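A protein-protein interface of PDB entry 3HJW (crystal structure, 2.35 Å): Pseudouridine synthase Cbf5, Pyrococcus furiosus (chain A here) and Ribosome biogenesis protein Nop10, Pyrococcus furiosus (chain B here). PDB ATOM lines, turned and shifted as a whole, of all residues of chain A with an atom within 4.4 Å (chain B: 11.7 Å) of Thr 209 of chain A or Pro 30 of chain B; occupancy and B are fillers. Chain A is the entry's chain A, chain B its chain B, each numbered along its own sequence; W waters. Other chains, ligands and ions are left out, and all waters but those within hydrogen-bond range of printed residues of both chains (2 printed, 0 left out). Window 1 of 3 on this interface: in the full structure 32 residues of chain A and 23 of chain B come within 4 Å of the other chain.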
ATOM      1  N   LEU A  44      10.201  24.236 -14.592  1.00  0.00           N
ATOM      2  CA  LEU A  44      11.305  23.289 -14.522  1.00  0.00           C
ATOM      3  C   LEU A  44      12.611  23.782 -15.140  1.00  0.00           C
ATOM      4  O   LEU A  44      12.624  24.351 -16.238  1.00  0.00           O
ATOM      5  CB  LEU A  44      10.927  21.960 -15.176  1.00  0.00           C
ATOM      6  CG  LEU A  44      11.882  20.794 -14.915  1.00  0.00           C
ATOM      7  CD1 LEU A  44      11.607  20.161 -13.531  1.00  0.00           C
ATOM      8  CD2 LEU A  44      11.749  19.755 -16.016  1.00  0.00           C
ATOM      9  N   ASP A  45      13.707  23.536 -14.423  1.00  0.00           N
ATOM     10  CA  ASP A  45      15.037  23.710 -14.968  1.00  0.00           C
ATOM     11  C   ASP A  45      15.454  22.370 -15.587  1.00  0.00           C
ATOM     12  O   ASP A  45      15.963  21.489 -14.880  1.00  0.00           O
ATOM     13  CB  ASP A  45      16.023  24.138 -13.861  1.00  0.00           C
ATOM     14  CG  ASP A  45      17.341  24.668 -14.413  1.00  0.00           C
ATOM     15  OD1 ASP A  45      17.594  24.498 -15.626  1.00  0.00           O
ATOM     16  OD2 ASP A  45      18.144  25.262 -13.643  1.00  0.00           O
ATOM     17  N   LYS A  46      15.237  22.218 -16.896  1.00  0.00           N
ATOM     18  CA  LYS A  46      15.618  20.993 -17.587  1.00  0.00           C
ATOM     19  C   LYS A  46      17.134  20.773 -17.556  1.00  0.00           C
ATOM     20  O   LYS A  46      17.894  21.673 -17.880  1.00  0.00           O
ATOM     21  CB  LYS A  46      15.119  20.983 -19.030  1.00  0.00           C
ATOM     22  CG  LYS A  46      15.411  19.676 -19.778  1.00  0.00           C
ATOM     23  CD  LYS A  46      15.197  19.843 -21.268  1.00  0.00           C
ATOM     24  CE  LYS A  46      15.713  18.659 -22.064  1.00  0.00           C
ATOM     25  NZ  LYS A  46      17.204  18.619 -22.090  1.00  0.00           N
ATOM     26  N   PRO A  47      17.572  19.577 -17.137  1.00  0.00           N
ATOM     27  CA  PRO A  47      18.981  19.215 -17.204  1.00  0.00           C
ATOM     28  C   PRO A  47      19.383  18.808 -18.620  1.00  0.00           C
ATOM     29  O   PRO A  47      18.529  18.382 -19.393  1.00  0.00           O
ATOM     30  CB  PRO A  47      19.059  18.007 -16.274  1.00  0.00           C
ATOM     31  CG  PRO A  47      17.720  17.346 -16.433  1.00  0.00           C
ATOM     32  CD  PRO A  47      16.751  18.494 -16.557  1.00  0.00           C
ATOM     33  N   PRO A  48      20.676  18.933 -18.961  1.00  0.00           N
ATOM     34  CA  PRO A  48      21.149  18.380 -20.229  1.00  0.00           C
ATOM     35  C   PRO A  48      21.117  16.853 -20.153  1.00  0.00           C
ATOM     36  O   PRO A  48      21.260  16.288 -19.064  1.00  0.00           O
ATOM     37  CB  PRO A  48      22.593  18.882 -20.311  1.00  0.00           C
ATOM     38  CG  PRO A  48      23.007  19.096 -18.877  1.00  0.00           C
ATOM     39  CD  PRO A  48      21.763  19.554 -18.177  1.00  0.00           C
ATOM     40  N   SER A  79      19.756  22.996 -21.522  1.00  0.00           N
ATOM     41  CA  SER A  79      19.166  23.105 -20.194  1.00  0.00           C
ATOM     42  C   SER A  79      18.255  24.337 -20.088  1.00  0.00           C
ATOM     43  O   SER A  79      18.208  25.158 -21.000  1.00  0.00           O
ATOM     44  CB  SER A  79      20.266  23.182 -19.128  1.00  0.00           C
ATOM     45  OG  SER A  79      20.881  24.466 -19.131  1.00  0.00           O
ATOM     46  N   ARG A 194      21.208  27.511 -23.273  1.00  0.00           N
ATOM     47  CA  ARG A 194      20.366  27.427 -22.100  1.00  0.00           C
ATOM     48  C   ARG A 194      19.175  28.373 -22.269  1.00  0.00           C
ATOM     49  O   ARG A 194      19.351  29.539 -22.599  1.00  0.00           O
ATOM     50  CB  ARG A 194      21.189  27.745 -20.837  1.00  0.00           C
ATOM     51  CG  ARG A 194      20.371  27.829 -19.564  1.00  0.00           C
ATOM     52  CD  ARG A 194      21.233  27.962 -18.339  1.00  0.00           C
ATOM     53  NE  ARG A 194      20.442  28.195 -17.138  1.00  0.00           N
ATOM     54  CZ  ARG A 194      19.797  27.250 -16.447  1.00  0.00           C
ATOM     55  NH1 ARG A 194      19.841  25.972 -16.829  1.00  0.00           N
ATOM     56  NH2 ARG A 194      19.101  27.582 -15.356  1.00  0.00           N
ATOM     57  N   ILE A 208      12.762  25.354 -10.704  1.00  0.00           N
ATOM     58  CA  ILE A 208      13.106  24.206  -9.867  1.00  0.00           C
ATOM     59  C   ILE A 208      13.722  23.046 -10.658  1.00  0.00           C
ATOM     60  O   ILE A 208      13.319  22.754 -11.790  1.00  0.00           O
ATOM     61  CB  ILE A 208      11.881  23.759  -9.007  1.00  0.00           C
ATOM     62  CG1 ILE A 208      12.311  22.819  -7.874  1.00  0.00           C
ATOM     63  CG2 ILE A 208      10.730  23.190  -9.899  1.00  0.00           C
ATOM     64  CD1 ILE A 208      11.170  22.323  -6.978  1.00  0.00           C
ATOM     65  N   THR A 209      14.723  22.409 -10.058  1.00  0.00           N
ATOM     66  CA  THR A 209      15.384  21.261 -10.669  1.00  0.00           C
ATOM     67  C   THR A 209      14.580  19.994 -10.420  1.00  0.00           C
ATOM     68  O   THR A 209      13.742  19.932  -9.507  1.00  0.00           O
ATOM     69  CB  THR A 209      16.811  21.068 -10.123  1.00  0.00           C
ATOM     70  OG1 THR A 209      16.748  20.814  -8.718  1.00  0.00           O
ATOM     71  CG2 THR A 209      17.682  22.307 -10.384  1.00  0.00           C
ATOM     72  N   LEU A 210      14.826  18.981 -11.244  1.00  0.00           N
ATOM     73  CA  LEU A 210      14.222  17.676 -11.045  1.00  0.00           C
ATOM     74  C   LEU A 210      14.481  17.145  -9.631  1.00  0.00           C
ATOM     75  O   LEU A 210      13.551  16.689  -8.952  1.00  0.00           O
ATOM     76  CB  LEU A 210      14.736  16.685 -12.098  1.00  0.00           C
ATOM     77  CG  LEU A 210      13.978  16.696 -13.425  1.00  0.00           C
ATOM     78  CD1 LEU A 210      14.685  15.851 -14.476  1.00  0.00           C
ATOM     79  CD2 LEU A 210      12.530  16.241 -13.225  1.00  0.00           C
ATOM     80  N   HIS A 211      15.733  17.229  -9.191  1.00  0.00           N
ATOM     81  CA  HIS A 211      16.121  16.764  -7.862  1.00  0.00           C
ATOM     82  C   HIS A 211      15.273  17.395  -6.792  1.00  0.00           C
ATOM     83  O   HIS A 211      14.696  16.683  -5.982  1.00  0.00           O
ATOM     84  CB  HIS A 211      17.589  17.053  -7.572  1.00  0.00           C
ATOM     85  CG  HIS A 211      18.525  16.497  -8.591  1.00  0.00           C
ATOM     86  ND1 HIS A 211      19.326  15.402  -8.347  1.00  0.00           N
ATOM     87  CD2 HIS A 211      18.800  16.893  -9.854  1.00  0.00           C
ATOM     88  CE1 HIS A 211      20.048  15.141  -9.422  1.00  0.00           C
ATOM     89  NE2 HIS A 211      19.751  16.036 -10.348  1.00  0.00           N
ATOM     90  N   ASP A 212      15.185  18.723  -6.791  1.00  0.00           N
ATOM     91  CA  ASP A 212      14.381  19.415  -5.783  1.00  0.00           C
ATOM     92  C   ASP A 212      12.906  19.062  -5.923  1.00  0.00           C
ATOM     93  O   ASP A 212      12.190  18.959  -4.929  1.00  0.00           O
ATOM     94  CB  ASP A 212      14.591  20.936  -5.833  1.00  0.00           C
ATOM     95  CG  ASP A 212      15.892  21.385  -5.133  1.00  0.00           C
ATOM     96  OD1 ASP A 212      16.389  20.673  -4.227  1.00  0.00           O
ATOM     97  OD2 ASP A 212      16.422  22.470  -5.484  1.00  0.00           O
ATOM     98  N   LEU A 213      12.459  18.865  -7.161  1.00  0.00           N
ATOM     99  CA  LEU A 213      11.077  18.519  -7.404  1.00  0.00           C
ATOM    100  C   LEU A 213      10.721  17.160  -6.788  1.00  0.00           C
ATOM    101  O   LEU A 213       9.718  17.048  -6.087  1.00  0.00           O
ATOM    102  CB  LEU A 213      10.742  18.547  -8.901  1.00  0.00           C
ATOM    103  CG  LEU A 213       9.285  18.197  -9.224  1.00  0.00           C
ATOM    104  CD1 LEU A 213       8.310  19.240  -8.644  1.00  0.00           C
ATOM    105  CD2 LEU A 213       9.082  18.023 -10.730  1.00  0.00           C
ATOM    106  N   PHE B   1      31.064  21.637 -20.014  1.00  0.00           N
ATOM    107  CA  PHE B   1      30.167  22.836 -20.037  1.00  0.00           C
ATOM    108  C   PHE B   1      30.905  24.072 -19.548  1.00  0.00           C
ATOM    109  O   PHE B   1      31.451  24.078 -18.446  1.00  0.00           O
ATOM    110  CB  PHE B   1      28.921  22.609 -19.183  1.00  0.00           C
ATOM    111  CG  PHE B   1      27.988  21.575 -19.738  1.00  0.00           C
ATOM    112  CD1 PHE B   1      27.757  20.384 -19.041  1.00  0.00           C
ATOM    113  CD2 PHE B   1      27.338  21.783 -20.954  1.00  0.00           C
ATOM    114  CE1 PHE B   1      26.892  19.415 -19.554  1.00  0.00           C
ATOM    115  CE2 PHE B   1      26.474  20.825 -21.477  1.00  0.00           C
ATOM    116  CZ  PHE B   1      26.251  19.639 -20.783  1.00  0.00           C
ATOM    117  N   ARG B   2      30.907  25.117 -20.365  1.00  0.00           N
ATOM    118  CA  ARG B   2      31.696  26.308 -20.072  1.00  0.00           C
ATOM    119  C   ARG B   2      30.882  27.464 -19.460  1.00  0.00           C
ATOM    120  O   ARG B   2      31.457  28.346 -18.805  1.00  0.00           O
ATOM    121  CB  ARG B   2      32.429  26.783 -21.334  1.00  0.00           C
ATOM    122  CG  ARG B   2      33.330  25.734 -21.998  1.00  0.00           C
ATOM    123  CD  ARG B   2      34.551  26.403 -22.619  1.00  0.00           C
ATOM    124  NE  ARG B   2      35.137  27.306 -21.627  1.00  0.00           N
ATOM    125  CZ  ARG B   2      35.681  28.488 -21.896  1.00  0.00           C
ATOM    126  NH1 ARG B   2      35.741  28.937 -23.151  1.00  0.00           N
ATOM    127  NH2 ARG B   2      36.159  29.226 -20.895  1.00  0.00           N
ATOM    128  N   ILE B   3      29.565  27.471 -19.686  1.00  0.00           N
ATOM    129  CA  ILE B   3      28.696  28.543 -19.178  1.00  0.00           C
ATOM    130  C   ILE B   3      28.569  28.495 -17.651  1.00  0.00           C
ATOM    131  O   ILE B   3      28.232  27.462 -17.070  1.00  0.00           O
ATOM    132  CB  ILE B   3      27.297  28.565 -19.872  1.00  0.00           C
ATOM    133  CG1 ILE B   3      27.452  28.716 -21.394  1.00  0.00           C
ATOM    134  CG2 ILE B   3      26.446  29.716 -19.338  1.00  0.00           C
ATOM    135  CD1 ILE B   3      26.138  28.705 -22.187  1.00  0.00           C
ATOM    136  N   ARG B   4      28.868  29.618 -17.012  1.00  0.00           N
ATOM    137  CA  ARG B   4      28.770  29.745 -15.557  1.00  0.00           C
ATOM    138  C   ARG B   4      27.853  30.912 -15.225  1.00  0.00           C
ATOM    139  O   ARG B   4      27.543  31.739 -16.091  1.00  0.00           O
ATOM    140  CB  ARG B   4      30.156  29.968 -14.932  1.00  0.00           C
ATOM    141  CG  ARG B   4      31.196  28.921 -15.318  1.00  0.00           C
ATOM    142  CD  ARG B   4      32.566  29.179 -14.688  1.00  0.00           C
ATOM    143  NE  ARG B   4      32.532  28.932 -13.248  1.00  0.00           N
ATOM    144  CZ  ARG B   4      32.674  27.733 -12.685  1.00  0.00           C
ATOM    145  NH1 ARG B   4      32.864  26.656 -13.440  1.00  0.00           N
ATOM    146  NH2 ARG B   4      32.607  27.612 -11.364  1.00  0.00           N
ATOM    147  N   LYS B   5      27.415  30.988 -13.972  1.00  0.00           N
ATOM    148  CA  LYS B   5      26.634  32.139 -13.528  1.00  0.00           C
ATOM    149  C   LYS B   5      26.864  32.448 -12.045  1.00  0.00           C
ATOM    150  O   LYS B   5      27.096  31.515 -11.270  1.00  0.00           O
ATOM    151  CB  LYS B   5      25.152  31.975 -13.898  1.00  0.00           C
ATOM    152  CG  LYS B   5      24.364  31.077 -12.996  1.00  0.00           C
ATOM    153  CD  LYS B   5      22.852  31.243 -13.201  1.00  0.00           C
ATOM    154  CE  LYS B   5      22.406  32.652 -12.946  1.00  0.00           C
ATOM    155  NZ  LYS B   5      20.923  32.781 -13.169  1.00  0.00           N
ATOM    156  N   TYR B  12      25.577  35.758 -16.208  1.00  0.00           N
ATOM    157  CA  TYR B  12      26.180  34.681 -16.970  1.00  0.00           C
ATOM    158  C   TYR B  12      27.575  35.098 -17.415  1.00  0.00           C
ATOM    159  O   TYR B  12      27.783  36.225 -17.863  1.00  0.00           O
ATOM    160  CB  TYR B  12      25.314  34.303 -18.177  1.00  0.00           C
ATOM    161  CG  TYR B  12      24.151  33.435 -17.790  1.00  0.00           C
ATOM    162  CD1 TYR B  12      22.890  33.983 -17.558  1.00  0.00           C
ATOM    163  CD2 TYR B  12      24.322  32.065 -17.608  1.00  0.00           C
ATOM    164  CE1 TYR B  12      21.817  33.179 -17.176  1.00  0.00           C
ATOM    165  CE2 TYR B  12      23.272  31.258 -17.223  1.00  0.00           C
ATOM    166  CZ  TYR B  12      22.019  31.818 -17.018  1.00  0.00           C
ATOM    167  OH  TYR B  12      20.997  30.995 -16.633  1.00  0.00           O
ATOM    168  N   LYS B  26      29.257  29.488 -10.381  1.00  0.00           N
ATOM    169  CA  LYS B  26      28.943  28.062 -10.488  1.00  0.00           C
ATOM    170  C   LYS B  26      28.541  27.705 -11.914  1.00  0.00           C
ATOM    171  O   LYS B  26      28.153  28.578 -12.683  1.00  0.00           O
ATOM    172  CB  LYS B  26      27.819  27.716  -9.516  1.00  0.00           C
ATOM    173  CG  LYS B  26      28.239  27.863  -8.055  1.00  0.00           C
ATOM    174  CD  LYS B  26      27.029  28.036  -7.143  1.00  0.00           C
ATOM    175  CE  LYS B  26      27.447  28.074  -5.664  1.00  0.00           C
ATOM    176  NZ  LYS B  26      26.258  28.106  -4.751  1.00  0.00           N
ATOM    177  N   VAL B  27      28.658  26.425 -12.271  1.00  0.00           N
ATOM    178  CA  VAL B  27      28.182  25.937 -13.573  1.00  0.00           C
ATOM    179  C   VAL B  27      26.661  26.200 -13.714  1.00  0.00           C
ATOM    180  O   VAL B  27      25.893  25.952 -12.790  1.00  0.00           O
ATOM    181  CB  VAL B  27      28.517  24.433 -13.780  1.00  0.00           C
ATOM    182  CG1 VAL B  27      28.190  23.984 -15.210  1.00  0.00           C
ATOM    183  CG2 VAL B  27      29.987  24.161 -13.494  1.00  0.00           C
ATOM    184  N   ALA B  28      26.251  26.711 -14.873  1.00  0.00           N
ATOM    185  CA  ALA B  28      24.879  27.178 -15.098  1.00  0.00           C
ATOM    186  C   ALA B  28      23.857  26.049 -15.233  1.00  0.00           C
ATOM    187  O   ALA B  28      22.689  26.206 -14.868  1.00  0.00           O
ATOM    188  CB  ALA B  28      24.833  28.056 -16.322  1.00  0.00           C
ATOM    189  N   HIS B  29      24.297  24.922 -15.776  1.00  0.00           N
ATOM    190  CA  HIS B  29      23.415  23.788 -16.013  1.00  0.00           C
ATOM    191  C   HIS B  29      23.148  23.005 -14.715  1.00  0.00           C
ATOM    192  O   HIS B  29      24.042  22.838 -13.884  1.00  0.00           O
ATOM    193  CB  HIS B  29      23.981  22.904 -17.137  1.00  0.00           C
ATOM    194  CG  HIS B  29      24.398  23.686 -18.351  1.00  0.00           C
ATOM    195  ND1 HIS B  29      23.557  23.909 -19.425  1.00  0.00           N
ATOM    196  CD2 HIS B  29      25.558  24.333 -18.643  1.00  0.00           C
ATOM    197  CE1 HIS B  29      24.187  24.637 -20.334  1.00  0.00           C
ATOM    198  NE2 HIS B  29      25.400  24.911 -19.883  1.00  0.00           N
ATOM    199  N   PRO B  30      21.899  22.562 -14.518  1.00  0.00           N
ATOM    200  CA  PRO B  30      21.589  21.785 -13.327  1.00  0.00           C
ATOM    201  C   PRO B  30      22.203  20.362 -13.414  1.00  0.00           C
ATOM    202  O   PRO B  30      22.501  19.891 -14.515  1.00  0.00           O
ATOM    203  CB  PRO B  30      20.056  21.738 -13.337  1.00  0.00           C
ATOM    204  CG  PRO B  30      19.685  21.853 -14.741  1.00  0.00           C
ATOM    205  CD  PRO B  30      20.717  22.741 -15.383  1.00  0.00           C
ATOM    206  N   PRO B  31      22.407  19.699 -12.262  1.00  0.00           N
ATOM    207  CA  PRO B  31      22.958  18.343 -12.285  1.00  0.00           C
ATOM    208  C   PRO B  31      22.078  17.360 -13.064  1.00  0.00           C
ATOM    209  O   PRO B  31      20.859  17.546 -13.174  1.00  0.00           O
ATOM    210  CB  PRO B  31      23.020  17.945 -10.806  1.00  0.00           C
ATOM    211  CG  PRO B  31      22.185  18.929 -10.071  1.00  0.00           C
ATOM    212  CD  PRO B  31      22.145  20.177 -10.891  1.00  0.00           C
ATOM    213  N   ARG B  32      22.708  16.324 -13.606  1.00  0.00           N
ATOM    214  CA  ARG B  32      22.009  15.295 -14.354  1.00  0.00           C
ATOM    215  C   ARG B  32      21.116  14.458 -13.432  1.00  0.00           C
ATOM    216  O   ARG B  32      21.417  14.291 -12.252  1.00  0.00           O
ATOM    217  CB  ARG B  32      23.024  14.464 -15.136  1.00  0.00           C
ATOM    218  CG  ARG B  32      24.009  15.379 -15.896  1.00  0.00           C
ATOM    219  CD  ARG B  32      24.941  14.640 -16.852  1.00  0.00           C
ATOM    220  NE  ARG B  32      24.337  14.381 -18.163  1.00  0.00           N
ATOM    221  CZ  ARG B  32      24.624  15.047 -19.282  1.00  0.00           C
ATOM    222  NH1 ARG B  32      25.512  16.033 -19.276  1.00  0.00           N
ATOM    223  NH2 ARG B  32      24.021  14.712 -20.419  1.00  0.00           N
ATOM    224  N   PHE B  33      19.989  13.991 -13.963  1.00  0.00           N
ATOM    225  CA  PHE B  33      18.995  13.279 -13.165  1.00  0.00           C
ATOM    226  C   PHE B  33      18.619  11.937 -13.796  1.00  0.00           C
ATOM    227  O   PHE B  33      18.379  11.859 -15.001  1.00  0.00           O
ATOM    228  CB  PHE B  33      17.738  14.147 -12.951  1.00  0.00           C
ATOM    229  CG  PHE B  33      16.665  13.481 -12.113  1.00  0.00           C
ATOM    230  CD1 PHE B  33      16.713  13.535 -10.722  1.00  0.00           C
ATOM    231  CD2 PHE B  33      15.611  12.802 -12.717  1.00  0.00           C
ATOM    232  CE1 PHE B  33      15.731  12.918  -9.943  1.00  0.00           C
ATOM    233  CE2 PHE B  33      14.614  12.184 -11.953  1.00  0.00           C
ATOM    234  CZ  PHE B  33      14.671  12.241 -10.564  1.00  0.00           C
ATOM    235  N   SER B  34      18.564  10.899 -12.966  1.00  0.00           N
ATOM    236  CA  SER B  34      18.109   9.564 -13.375  1.00  0.00           C
ATOM    237  C   SER B  34      16.726   9.278 -12.793  1.00  0.00           C
ATOM    238  O   SER B  34      16.499   9.506 -11.597  1.00  0.00           O
ATOM    239  CB  SER B  34      19.066   8.478 -12.867  1.00  0.00           C
ATOM    240  OG  SER B  34      20.419   8.765 -13.196  1.00  0.00           O
ATOM    241  N   ASP B  37      17.240   7.149  -9.992  1.00  0.00           N
ATOM    242  CA  ASP B  37      17.671   7.967  -8.849  1.00  0.00           C
ATOM    243  C   ASP B  37      18.213   7.134  -7.672  1.00  0.00           C
ATOM    244  O   ASP B  37      17.611   7.117  -6.593  1.00  0.00           O
ATOM    245  CB  ASP B  37      16.523   8.893  -8.399  1.00  0.00           C
ATOM    246  CG  ASP B  37      17.008  10.063  -7.555  1.00  0.00           C
ATOM    247  OD1 ASP B  37      18.119  10.583  -7.822  1.00  0.00           O
ATOM    248  OD2 ASP B  37      16.273  10.462  -6.625  1.00  0.00           O
ATOM    249  N   ARG B  43      20.757  11.401  -0.628  1.00  0.00           N
ATOM    250  CA  ARG B  43      20.717  12.812  -0.988  1.00  0.00           C
ATOM    251  C   ARG B  43      19.632  13.530  -0.181  1.00  0.00           C
ATOM    252  O   ARG B  43      19.861  14.629   0.333  1.00  0.00           O
ATOM    253  CB  ARG B  43      20.493  12.995  -2.495  1.00  0.00           C
ATOM    254  CG  ARG B  43      20.351  14.447  -2.928  1.00  0.00           C
ATOM    255  CD  ARG B  43      19.897  14.604  -4.379  1.00  0.00           C
ATOM    256  NE  ARG B  43      18.485  14.275  -4.580  1.00  0.00           N
ATOM    257  CZ  ARG B  43      18.041  13.306  -5.381  1.00  0.00           C
ATOM    258  NH1 ARG B  43      18.892  12.563  -6.076  1.00  0.00           N
ATOM    259  NH2 ARG B  43      16.736  13.087  -5.500  1.00  0.00           N
ATOM    260  N   ARG B  44      18.465  12.901  -0.056  1.00  0.00           N
ATOM    261  CA  ARG B  44      17.380  13.442   0.772  1.00  0.00           C
ATOM    262  C   ARG B  44      17.757  13.624   2.242  1.00  0.00           C
ATOM    263  O   ARG B  44      17.273  14.547   2.888  1.00  0.00           O
ATOM    264  CB  ARG B  44      16.120  12.588   0.659  1.00  0.00           C
ATOM    265  CG  ARG B  44      15.053  13.191  -0.222  1.00  0.00           C
ATOM    266  CD  ARG B  44      13.896  12.236  -0.466  1.00  0.00           C
ATOM    267  NE  ARG B  44      14.008  11.633  -1.789  1.00  0.00           N
ATOM    268  CZ  ARG B  44      14.234  10.349  -2.024  1.00  0.00           C
ATOM    269  NH1 ARG B  44      14.350   9.502  -1.020  1.00  0.00           N
ATOM    270  NH2 ARG B  44      14.334   9.912  -3.269  1.00  0.00           N
ATOM    271  N   TRP B  46      20.829  14.328   3.361  1.00  0.00           N
ATOM    272  CA  TRP B  46      21.664  15.532   3.320  1.00  0.00           C
ATOM    273  C   TRP B  46      20.800  16.789   3.226  1.00  0.00           C
ATOM    274  O   TRP B  46      21.006  17.743   3.980  1.00  0.00           O
ATOM    275  CB  TRP B  46      22.630  15.443   2.134  1.00  0.00           C
ATOM    276  CG  TRP B  46      23.167  16.748   1.619  1.00  0.00           C
ATOM    277  CD1 TRP B  46      24.078  17.567   2.232  1.00  0.00           C
ATOM    278  CD2 TRP B  46      22.860  17.364   0.362  1.00  0.00           C
ATOM    279  NE1 TRP B  46      24.345  18.655   1.441  1.00  0.00           N
ATOM    280  CE2 TRP B  46      23.609  18.561   0.289  1.00  0.00           C
ATOM    281  CE3 TRP B  46      22.019  17.022  -0.711  1.00  0.00           C
ATOM    282  CZ2 TRP B  46      23.542  19.427  -0.816  1.00  0.00           C
ATOM    283  CZ3 TRP B  46      21.948  17.888  -1.814  1.00  0.00           C
ATOM    284  CH2 TRP B  46      22.709  19.075  -1.853  1.00  0.00           C
ATOM    285  N   LYS B  47      19.823  16.757   2.316  1.00  0.00           N
ATOM    286  CA  LYS B  47      18.928  17.886   2.057  1.00  0.00           C
ATOM    287  C   LYS B  47      18.032  18.214   3.250  1.00  0.00           C
ATOM    288  O   LYS B  47      17.744  19.391   3.502  1.00  0.00           O
ATOM    289  CB  LYS B  47      18.069  17.624   0.810  1.00  0.00           C
ATOM    290  CG  LYS B  47      17.417  18.877   0.234  1.00  0.00           C
ATOM    291  CD  LYS B  47      16.845  18.649  -1.162  1.00  0.00           C
ATOM    292  CE  LYS B  47      17.933  18.491  -2.235  1.00  0.00           C
ATOM    293  NZ  LYS B  47      17.319  18.225  -3.573  1.00  0.00           N
ATOM    294  N   LEU B  51      17.871  21.795   5.285  1.00  0.00           N
ATOM    295  CA  LEU B  51      16.643  22.573   5.177  1.00  0.00           C
ATOM    296  C   LEU B  51      16.037  22.840   6.551  1.00  0.00           C
ATOM    297  O   LEU B  51      15.015  23.515   6.669  1.00  0.00           O
ATOM    298  CB  LEU B  51      15.629  21.851   4.287  1.00  0.00           C
ATOM    299  CG  LEU B  51      15.828  21.997   2.777  1.00  0.00           C
ATOM    300  CD1 LEU B  51      14.767  21.216   2.018  1.00  0.00           C
ATOM    301  CD2 LEU B  51      15.815  23.462   2.372  1.00  0.00           C
HETATM  302  O   HOH W   1      20.602  25.194 -13.077  1.00  0.00           O
HETATM  303  O   HOH W   2      18.852  18.645 -12.109  1.00  0.00           O
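Pro 47 of chain A touches Pro 30 of chain B (CA to CG, 3.7 Å). CB of Pro 47 of chain A touches O of Pro 31 of chain B, 3.6 Å away. Pro 30 of chain B touches Ser 79 of chain A. NH1 of Arg 194 of chain A touches CD of Pro 30 of chain B (3.6 Å). Pro 30 of chain B touches Thr 209 of chain A. Leu 210 of chain A touches Phe 33 of chain B (CD1 to CD2, 3.6 Å). NE2 of His 211 of chain A touches CB of Phe 33 of chain B, 3.8 Å away.
Hydrophobic or aromatic side chains of chain B within 4 Å of the printed part of chain A: Phe 1, Tyr 12, His 29, Pro 30, Pro 31 and Phe 33. Of the 13 printed residues of chain A, 10 touch a printed residue of chain B. Hydrophobic or aromatic side chains of chain A within 4 Å of the printed part of chain B: Pro 47, Pro 48, Leu 210 and His 211. Among the printed residues, 20 pairs touch across the chains. Among the printed residues, Asp or Glu carboxylates within 4 Å of a Lys or Arg side-chain nitrogen of the other chain: Asp 212 of chain A with Lys 47 of chain B.
OD1 of Asp 37 of chain B is in salt-bridge range of NH1 of Arg 43 of chain B (2.8 Å). The backbone NH (N) of Asp 45 of chain A sits at hydrogen-bond distance from the backbone carbonyl oxygen (O) of Ile 208 of chain A. The side-chain hydroxyl of Thr 209 of chain A sits at hydrogen-bond distance from the backbone NH of Asp 212 of chain A (3.2 Å). NH1 of Arg 194 of chain A sits at hydrogen-bond distance from OG of Ser 79 of chain A (2.9 Å).
Water W2 bridges O of Pro 31 of chain B (2.5 Å) and NE2 of His 211 of chain A (3.3 Å). Water W1 lies within hydrogen-bond range of the side-chain carboxylate of Asp 45 of chain A (2.5 Å) and the backbone carbonyl oxygen of Ala 28 of chain B (2.9 Å).
The side-chain hydroxyl (OG) of Ser 79 of chain A lies within hydrogen-bond range of a ring nitrogen (ND1) of His 29 of chain B (2.7 Å). The guanidinium group (NE) of Arg 194 of chain A is in hydrogen-bond range of the side-chain hydroxyl (OH) of Tyr 12 of chain B (2.9 Å). NE2 of His 211 of chain A sits at hydrogen-bond distance from O of Pro 31 of chain B (3.4 Å). O of Ala 28 of chain B lies close to NH1 of Arg 194 of chain A (3.5 Å). A ring nitrogen (NE2) of His 211 of chain A lies within hydrogen-bond range of the backbone carbonyl oxygen (O) of Arg 32 of chain B, at 3.1 Å. The side-chain carboxylate (OD1) of Asp 212 of chain A is in salt-bridge range of the side-chain amino group (NZ) of Lys 47 of chain B, 2.7 Å away. O of Pro 48 of chain A is in hydrogen-bond range of NH2 of Arg 32 of chain B (3.5 Å).
Of the printed residues of chain B, Arg 194 of chain A touches Tyr 12, Ala 28 and Pro 30. Thr 209 of chain A touches just one residue of chain B: Pro 30 (3.8 Å). Leu 210 of chain A touches just one residue of chain B: Phe 33 (3.6 Å). His 211 of chain A touches five residues of chain B. Printed residues of chain A within 4 Å of Phe 1 of chain B: Pro 48. Printed residues of chain A within 4 Å of Tyr 12 of chain B: Arg 194 (2.9 Å). Printed residues of chain A within 4 Å of Ala 28 of chain B: Arg 194 (3.5 Å). Of chain A, only Asp 45 (3.5 Å), Lys 46 (3.6 Å), Pro 47 (3.7 Å), Pro 48 (3.8 Å), Ser 79 (3.8 Å), Arg 194 (3.6 Å) and Thr 209 (3.8 Å) come within 4 Å of Pro 30 of chain B. Of the printed residues of chain A, Arg 32 of chain B touches Pro 48 (3.5 Å) and His 211 (3.1 Å). The nearest printed residue of chain A that does not touch Lys 47 of chain B is Thr 209 of chain A (5.8 Å).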
